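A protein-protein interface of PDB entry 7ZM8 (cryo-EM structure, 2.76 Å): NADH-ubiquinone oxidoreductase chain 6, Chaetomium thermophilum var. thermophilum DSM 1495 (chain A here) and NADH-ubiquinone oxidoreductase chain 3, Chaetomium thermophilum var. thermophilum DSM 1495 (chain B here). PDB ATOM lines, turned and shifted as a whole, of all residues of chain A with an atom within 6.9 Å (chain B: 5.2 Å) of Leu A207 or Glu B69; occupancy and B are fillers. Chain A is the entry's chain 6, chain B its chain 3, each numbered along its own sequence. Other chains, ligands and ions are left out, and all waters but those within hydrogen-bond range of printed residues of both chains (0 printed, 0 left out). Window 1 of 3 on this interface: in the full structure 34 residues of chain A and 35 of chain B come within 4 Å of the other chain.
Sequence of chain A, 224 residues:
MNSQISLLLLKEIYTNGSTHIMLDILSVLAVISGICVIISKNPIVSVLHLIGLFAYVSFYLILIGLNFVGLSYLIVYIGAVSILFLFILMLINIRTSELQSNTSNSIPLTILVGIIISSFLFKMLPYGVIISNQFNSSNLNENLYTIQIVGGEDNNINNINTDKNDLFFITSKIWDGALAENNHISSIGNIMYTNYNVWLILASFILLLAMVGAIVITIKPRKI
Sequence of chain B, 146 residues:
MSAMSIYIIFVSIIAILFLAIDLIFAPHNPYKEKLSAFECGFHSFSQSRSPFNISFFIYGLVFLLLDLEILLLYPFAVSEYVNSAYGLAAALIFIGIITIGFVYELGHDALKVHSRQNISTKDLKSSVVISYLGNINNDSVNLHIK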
ATOM      1  N   LEU A 200       1.596 -15.806 -35.299  1.00  0.00           N
ATOM      2  CA  LEU A 200       2.280 -16.395 -34.122  1.00  0.00           C
ATOM      3  C   LEU A 200       1.529 -15.991 -32.855  1.00  0.00           C
ATOM      4  O   LEU A 200       1.350 -16.842 -31.985  1.00  0.00           O
ATOM      5  CB  LEU A 200       3.710 -15.848 -34.094  1.00  0.00           C
ATOM      6  CG  LEU A 200       4.669 -16.505 -33.104  1.00  0.00           C
ATOM      7  CD1 LEU A 200       4.938 -17.951 -33.486  1.00  0.00           C
ATOM      8  CD2 LEU A 200       5.968 -15.722 -33.039  1.00  0.00           C
ATOM      9  N   LEU A 202      -1.643 -15.233 -32.535  1.00  0.00           N
ATOM     10  CA  LEU A 202      -2.991 -15.832 -32.428  1.00  0.00           C
ATOM     11  C   LEU A 202      -2.854 -17.318 -32.139  1.00  0.00           C
ATOM     12  O   LEU A 202      -3.727 -17.863 -31.445  1.00  0.00           O
ATOM     13  CB  LEU A 202      -3.687 -15.653 -33.778  1.00  0.00           C
ATOM     14  CG  LEU A 202      -4.555 -14.406 -33.929  1.00  0.00           C
ATOM     15  CD1 LEU A 202      -5.157 -14.342 -35.326  1.00  0.00           C
ATOM     16  CD2 LEU A 202      -5.653 -14.393 -32.882  1.00  0.00           C
ATOM     17  N   ALA A 203      -1.787 -17.935 -32.649  1.00  0.00           N
ATOM     18  CA  ALA A 203      -1.545 -19.341 -32.364  1.00  0.00           C
ATOM     19  C   ALA A 203      -1.069 -19.546 -30.935  1.00  0.00           C
ATOM     20  O   ALA A 203      -1.413 -20.549 -30.299  1.00  0.00           O
ATOM     21  CB  ALA A 203      -0.529 -19.898 -33.354  1.00  0.00           C
ATOM     22  N   SER A 204      -0.267 -18.619 -30.417  1.00  0.00           N
ATOM     23  CA  SER A 204       0.157 -18.710 -29.025  1.00  0.00           C
ATOM     24  C   SER A 204      -1.037 -18.648 -28.085  1.00  0.00           C
ATOM     25  O   SER A 204      -1.045 -19.294 -27.033  1.00  0.00           O
ATOM     26  CB  SER A 204       1.151 -17.594 -28.708  1.00  0.00           C
ATOM     27  OG  SER A 204       0.521 -16.330 -28.757  1.00  0.00           O
ATOM     28  N   PHE A 205      -2.051 -17.865 -28.443  1.00  0.00           N
ATOM     29  CA  PHE A 205      -3.255 -17.801 -27.633  1.00  0.00           C
ATOM     30  C   PHE A 205      -4.142 -19.024 -27.824  1.00  0.00           C
ATOM     31  O   PHE A 205      -4.892 -19.382 -26.913  1.00  0.00           O
ATOM     32  CB  PHE A 205      -4.018 -16.513 -27.945  1.00  0.00           C
ATOM     33  CG  PHE A 205      -3.578 -15.342 -27.117  1.00  0.00           C
ATOM     34  CD1 PHE A 205      -4.128 -15.113 -25.869  1.00  0.00           C
ATOM     35  CD2 PHE A 205      -2.605 -14.478 -27.577  1.00  0.00           C
ATOM     36  CE1 PHE A 205      -3.724 -14.039 -25.107  1.00  0.00           C
ATOM     37  CE2 PHE A 205      -2.193 -13.404 -26.815  1.00  0.00           C
ATOM     38  CZ  PHE A 205      -2.753 -13.184 -25.581  1.00  0.00           C
ATOM     39  N   ILE A 206      -4.072 -19.676 -28.987  1.00  0.00           N
ATOM     40  CA  ILE A 206      -4.803 -20.926 -29.189  1.00  0.00           C
ATOM     41  C   ILE A 206      -4.194 -22.037 -28.348  1.00  0.00           C
ATOM     42  O   ILE A 206      -4.913 -22.826 -27.728  1.00  0.00           O
ATOM     43  CB  ILE A 206      -4.831 -21.298 -30.683  1.00  0.00           C
ATOM     44  CG1 ILE A 206      -5.895 -20.489 -31.417  1.00  0.00           C
ATOM     45  CG2 ILE A 206      -5.096 -22.776 -30.874  1.00  0.00           C
ATOM     46  CD1 ILE A 206      -5.928 -20.745 -32.894  1.00  0.00           C
ATOM     47  N   LEU A 207      -2.863 -22.124 -28.321  1.00  0.00           N
ATOM     48  CA  LEU A 207      -2.191 -23.089 -27.456  1.00  0.00           C
ATOM     49  C   LEU A 207      -2.438 -22.776 -25.989  1.00  0.00           C
ATOM     50  O   LEU A 207      -2.606 -23.685 -25.171  1.00  0.00           O
ATOM     51  CB  LEU A 207      -0.693 -23.096 -27.750  1.00  0.00           C
ATOM     52  CG  LEU A 207      -0.246 -23.603 -29.118  1.00  0.00           C
ATOM     53  CD1 LEU A 207       1.079 -22.970 -29.502  1.00  0.00           C
ATOM     54  CD2 LEU A 207      -0.135 -25.109 -29.111  1.00  0.00           C
ATOM     55  N   LEU A 208      -2.441 -21.491 -25.639  1.00  0.00           N
ATOM     56  CA  LEU A 208      -2.738 -21.072 -24.275  1.00  0.00           C
ATOM     57  C   LEU A 208      -4.138 -21.499 -23.855  1.00  0.00           C
ATOM     58  O   LEU A 208      -4.356 -21.891 -22.705  1.00  0.00           O
ATOM     59  CB  LEU A 208      -2.579 -19.556 -24.171  1.00  0.00           C
ATOM     60  CG  LEU A 208      -2.610 -18.882 -22.807  1.00  0.00           C
ATOM     61  CD1 LEU A 208      -1.450 -19.345 -21.975  1.00  0.00           C
ATOM     62  CD2 LEU A 208      -2.557 -17.394 -22.989  1.00  0.00           C
ATOM     63  N   LEU A 209      -5.105 -21.415 -24.771  1.00  0.00           N
ATOM     64  CA  LEU A 209      -6.461 -21.858 -24.474  1.00  0.00           C
ATOM     65  C   LEU A 209      -6.533 -23.374 -24.325  1.00  0.00           C
ATOM     66  O   LEU A 209      -7.239 -23.882 -23.449  1.00  0.00           O
ATOM     67  CB  LEU A 209      -7.411 -21.380 -25.568  1.00  0.00           C
ATOM     68  CG  LEU A 209      -8.878 -21.782 -25.454  1.00  0.00           C
ATOM     69  CD1 LEU A 209      -9.533 -21.056 -24.309  1.00  0.00           C
ATOM     70  CD2 LEU A 209      -9.602 -21.496 -26.751  1.00  0.00           C
ATOM     71  N   ALA A 210      -5.822 -24.110 -25.176  1.00  0.00           N
ATOM     72  CA  ALA A 210      -5.828 -25.561 -25.076  1.00  0.00           C
ATOM     73  C   ALA A 210      -5.145 -26.042 -23.806  1.00  0.00           C
ATOM     74  O   ALA A 210      -5.374 -27.175 -23.372  1.00  0.00           O
ATOM     75  CB  ALA A 210      -5.163 -26.172 -26.307  1.00  0.00           C
ATOM     76  N   MET A 211      -4.301 -25.208 -23.204  1.00  0.00           N
ATOM     77  CA  MET A 211      -3.673 -25.560 -21.938  1.00  0.00           C
ATOM     78  C   MET A 211      -4.623 -25.342 -20.772  1.00  0.00           C
ATOM     79  O   MET A 211      -4.902 -26.268 -20.006  1.00  0.00           O
ATOM     80  CB  MET A 211      -2.402 -24.739 -21.742  1.00  0.00           C
ATOM     81  CG  MET A 211      -1.771 -24.891 -20.373  1.00  0.00           C
ATOM     82  SD  MET A 211      -0.877 -26.441 -20.201  1.00  0.00           S
ATOM     83  CE  MET A 211       0.606 -26.060 -21.124  1.00  0.00           C
ATOM     84  N   VAL A 212      -5.124 -24.118 -20.628  1.00  0.00           N
ATOM     85  CA  VAL A 212      -6.003 -23.787 -19.516  1.00  0.00           C
ATOM     86  C   VAL A 212      -7.304 -24.572 -19.605  1.00  0.00           C
ATOM     87  O   VAL A 212      -7.787 -25.114 -18.605  1.00  0.00           O
ATOM     88  CB  VAL A 212      -6.255 -22.270 -19.493  1.00  0.00           C
ATOM     89  CG1 VAL A 212      -7.374 -21.924 -18.531  1.00  0.00           C
ATOM     90  CG2 VAL A 212      -4.984 -21.540 -19.136  1.00  0.00           C
ATOM     91  N   LEU B  65       1.592 -29.683 -26.076  1.00  0.00           N
ATOM     92  CA  LEU B  65       1.532 -28.241 -26.243  1.00  0.00           C
ATOM     93  C   LEU B  65       2.913 -27.604 -26.177  1.00  0.00           C
ATOM     94  O   LEU B  65       3.241 -26.755 -27.011  1.00  0.00           O
ATOM     95  CB  LEU B  65       0.600 -27.643 -25.194  1.00  0.00           C
ATOM     96  CG  LEU B  65      -0.868 -28.007 -25.410  1.00  0.00           C
ATOM     97  CD1 LEU B  65      -1.743 -27.262 -24.432  1.00  0.00           C
ATOM     98  CD2 LEU B  65      -1.310 -27.743 -26.839  1.00  0.00           C
ATOM     99  N   LEU B  66       3.739 -28.003 -25.206  1.00  0.00           N
ATOM    100  CA  LEU B  66       5.093 -27.466 -25.114  1.00  0.00           C
ATOM    101  C   LEU B  66       5.978 -27.937 -26.258  1.00  0.00           C
ATOM    102  O   LEU B  66       6.865 -27.199 -26.692  1.00  0.00           O
ATOM    103  CB  LEU B  66       5.729 -27.839 -23.775  1.00  0.00           C
ATOM    104  CG  LEU B  66       5.440 -26.994 -22.534  1.00  0.00           C
ATOM    105  CD1 LEU B  66       5.979 -25.587 -22.718  1.00  0.00           C
ATOM    106  CD2 LEU B  66       3.968 -26.946 -22.214  1.00  0.00           C
ATOM    107  N   ASP B  67       5.771 -29.162 -26.742  1.00  0.00           N
ATOM    108  CA  ASP B  67       6.534 -29.649 -27.887  1.00  0.00           C
ATOM    109  C   ASP B  67       6.255 -28.810 -29.127  1.00  0.00           C
ATOM    110  O   ASP B  67       7.173 -28.503 -29.895  1.00  0.00           O
ATOM    111  CB  ASP B  67       6.198 -31.118 -28.146  1.00  0.00           C
ATOM    112  CG  ASP B  67       7.300 -31.858 -28.859  1.00  0.00           C
ATOM    113  OD1 ASP B  67       8.482 -31.499 -28.689  1.00  0.00           O
ATOM    114  OD2 ASP B  67       6.980 -32.813 -29.588  1.00  0.00           O
ATOM    115  N   LEU B  68       4.992 -28.438 -29.344  1.00  0.00           N
ATOM    116  CA  LEU B  68       4.655 -27.549 -30.453  1.00  0.00           C
ATOM    117  C   LEU B  68       5.271 -26.166 -30.270  1.00  0.00           C
ATOM    118  O   LEU B  68       5.774 -25.574 -31.230  1.00  0.00           O
ATOM    119  CB  LEU B  68       3.138 -27.440 -30.600  1.00  0.00           C
ATOM    120  CG  LEU B  68       2.425 -28.461 -31.491  1.00  0.00           C
ATOM    121  CD1 LEU B  68       0.924 -28.375 -31.307  1.00  0.00           C
ATOM    122  CD2 LEU B  68       2.791 -28.270 -32.949  1.00  0.00           C
ATOM    123  N   GLU B  69       5.240 -25.631 -29.048  1.00  0.00           N
ATOM    124  CA  GLU B  69       5.766 -24.286 -28.825  1.00  0.00           C
ATOM    125  C   GLU B  69       7.280 -24.241 -28.993  1.00  0.00           C
ATOM    126  O   GLU B  69       7.812 -23.294 -29.579  1.00  0.00           O
ATOM    127  CB  GLU B  69       5.374 -23.779 -27.441  1.00  0.00           C
ATOM    128  CG  GLU B  69       3.912 -23.452 -27.280  1.00  0.00           C
ATOM    129  CD  GLU B  69       3.350 -23.960 -25.966  1.00  0.00           C
ATOM    130  OE1 GLU B  69       2.152 -24.311 -25.917  1.00  0.00           O
ATOM    131  OE2 GLU B  69       4.106 -24.009 -24.978  1.00  0.00           O
ATOM    132  N   ILE B  70       7.990 -25.245 -28.472  1.00  0.00           N
ATOM    133  CA  ILE B  70       9.435 -25.311 -28.661  1.00  0.00           C
ATOM    134  C   ILE B  70       9.767 -25.502 -30.134  1.00  0.00           C
ATOM    135  O   ILE B  70      10.758 -24.966 -30.637  1.00  0.00           O
ATOM    136  CB  ILE B  70      10.043 -26.422 -27.779  1.00  0.00           C
ATOM    137  CG1 ILE B  70      10.229 -25.926 -26.346  1.00  0.00           C
ATOM    138  CG2 ILE B  70      11.377 -26.916 -28.325  1.00  0.00           C
ATOM    139  CD1 ILE B  70      11.213 -24.793 -26.227  1.00  0.00           C
ATOM    140  N   LEU B  71       8.933 -26.258 -30.850  1.00  0.00           N
ATOM    141  CA  LEU B  71       9.124 -26.428 -32.286  1.00  0.00           C
ATOM    142  C   LEU B  71       9.030 -25.098 -33.017  1.00  0.00           C
ATOM    143  O   LEU B  71       9.821 -24.823 -33.924  1.00  0.00           O
ATOM    144  CB  LEU B  71       8.090 -27.404 -32.842  1.00  0.00           C
ATOM    145  CG  LEU B  71       8.222 -27.720 -34.336  1.00  0.00           C
ATOM    146  CD1 LEU B  71       9.545 -28.406 -34.644  1.00  0.00           C
ATOM    147  CD2 LEU B  71       7.042 -28.526 -34.847  1.00  0.00           C
ATOM    148  N   LEU B  72       8.060 -24.261 -32.645  1.00  0.00           N
ATOM    149  CA  LEU B  72       7.869 -22.981 -33.312  1.00  0.00           C
ATOM    150  C   LEU B  72       9.023 -22.021 -33.063  1.00  0.00           C
ATOM    151  O   LEU B  72       9.149 -21.026 -33.779  1.00  0.00           O
ATOM    152  CB  LEU B  72       6.556 -22.346 -32.858  1.00  0.00           C
ATOM    153  CG  LEU B  72       5.256 -23.012 -33.313  1.00  0.00           C
ATOM    154  CD1 LEU B  72       4.210 -22.897 -32.229  1.00  0.00           C
ATOM    155  CD2 LEU B  72       4.734 -22.426 -34.609  1.00  0.00           C
ATOM    156  N   LEU B  73       9.865 -22.300 -32.072  1.00  0.00           N
ATOM    157  CA  LEU B  73      11.035 -21.485 -31.784  1.00  0.00           C
ATOM    158  C   LEU B  73      12.275 -21.916 -32.555  1.00  0.00           C
ATOM    159  O   LEU B  73      13.202 -21.116 -32.701  1.00  0.00           O
ATOM    160  CB  LEU B  73      11.337 -21.524 -30.287  1.00  0.00           C
ATOM    161  CG  LEU B  73      10.509 -20.605 -29.401  1.00  0.00           C
ATOM    162  CD1 LEU B  73      10.873 -20.840 -27.959  1.00  0.00           C
ATOM    163  CD2 LEU B  73      10.738 -19.154 -29.793  1.00  0.00           C
ATOM    164  N   PHE B  94       6.307 -14.095 -27.831  1.00  0.00           N
ATOM    165  CA  PHE B  94       5.802 -15.455 -27.966  1.00  0.00           C
ATOM    166  C   PHE B  94       6.257 -16.333 -26.809  1.00  0.00           C
ATOM    167  O   PHE B  94       5.486 -17.153 -26.301  1.00  0.00           O
ATOM    168  CB  PHE B  94       6.245 -16.058 -29.297  1.00  0.00           C
ATOM    169  CG  PHE B  94       5.856 -17.491 -29.461  1.00  0.00           C
ATOM    170  CD1 PHE B  94       4.542 -17.838 -29.691  1.00  0.00           C
ATOM    171  CD2 PHE B  94       6.797 -18.495 -29.374  1.00  0.00           C
ATOM    172  CE1 PHE B  94       4.180 -19.155 -29.839  1.00  0.00           C
ATOM    173  CE2 PHE B  94       6.430 -19.813 -29.516  1.00  0.00           C
ATOM    174  CZ  PHE B  94       5.121 -20.138 -29.749  1.00  0.00           C
ATOM    175  N   ILE B  98       3.542 -18.239 -23.689  1.00  0.00           N
ATOM    176  CA  ILE B  98       3.660 -19.693 -23.378  1.00  0.00           C
ATOM    177  C   ILE B  98       4.141 -19.906 -21.935  1.00  0.00           C
ATOM    178  O   ILE B  98       3.670 -20.864 -21.303  1.00  0.00           O
ATOM    179  CB  ILE B  98       4.463 -20.455 -24.458  1.00  0.00           C
ATOM    180  CG1 ILE B  98       5.974 -20.238 -24.359  1.00  0.00           C
ATOM    181  CG2 ILE B  98       3.937 -20.116 -25.843  1.00  0.00           C
ATOM    182  CD1 ILE B  98       6.731 -20.627 -25.607  1.00  0.00           C
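Among the printed residues, merely in contact across the chains: Leu A200 with Phe B94, Ser A204 with Phe B94, Leu A207 with Leu B65, Leu A207 with Glu B69, Ala A210 with Leu B65, Met A211 with Leu B65 and Met A211 with Leu B66.
Of the 12 printed residues of chain A, 5 touch a printed residue of chain B. Printed residues of chain B that touch a printed residue of chain A: Leu B65, Leu B66, Glu B69 and Phe B94. Along chain B the printed residues that touch a printed residue of chain A span positions 65 to 94. Among the printed residues, no Asp or Glu carboxylate lies within 4 Å of a Lys or Arg side-chain nitrogen of the other chain.
The backbone carbonyl oxygen (O) of Leu A200 lies close to the side-chain hydroxyl (OG) of Ser A204 (3.4 Å).
Of the printed residues of chain B, Ser A204 touches Phe B94. Of the printed residues of chain A, Leu B65 touches Leu A207, Ala A210 and Met A211. Ile B70 touches none of the printed residues of chain A. The nearest residue of chain B that does not touch Leu A207 is Leu B68 (4.1 Å). The nearest residue of chain A that does not touch Glu B69 is Met A211 (5.3 Å).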
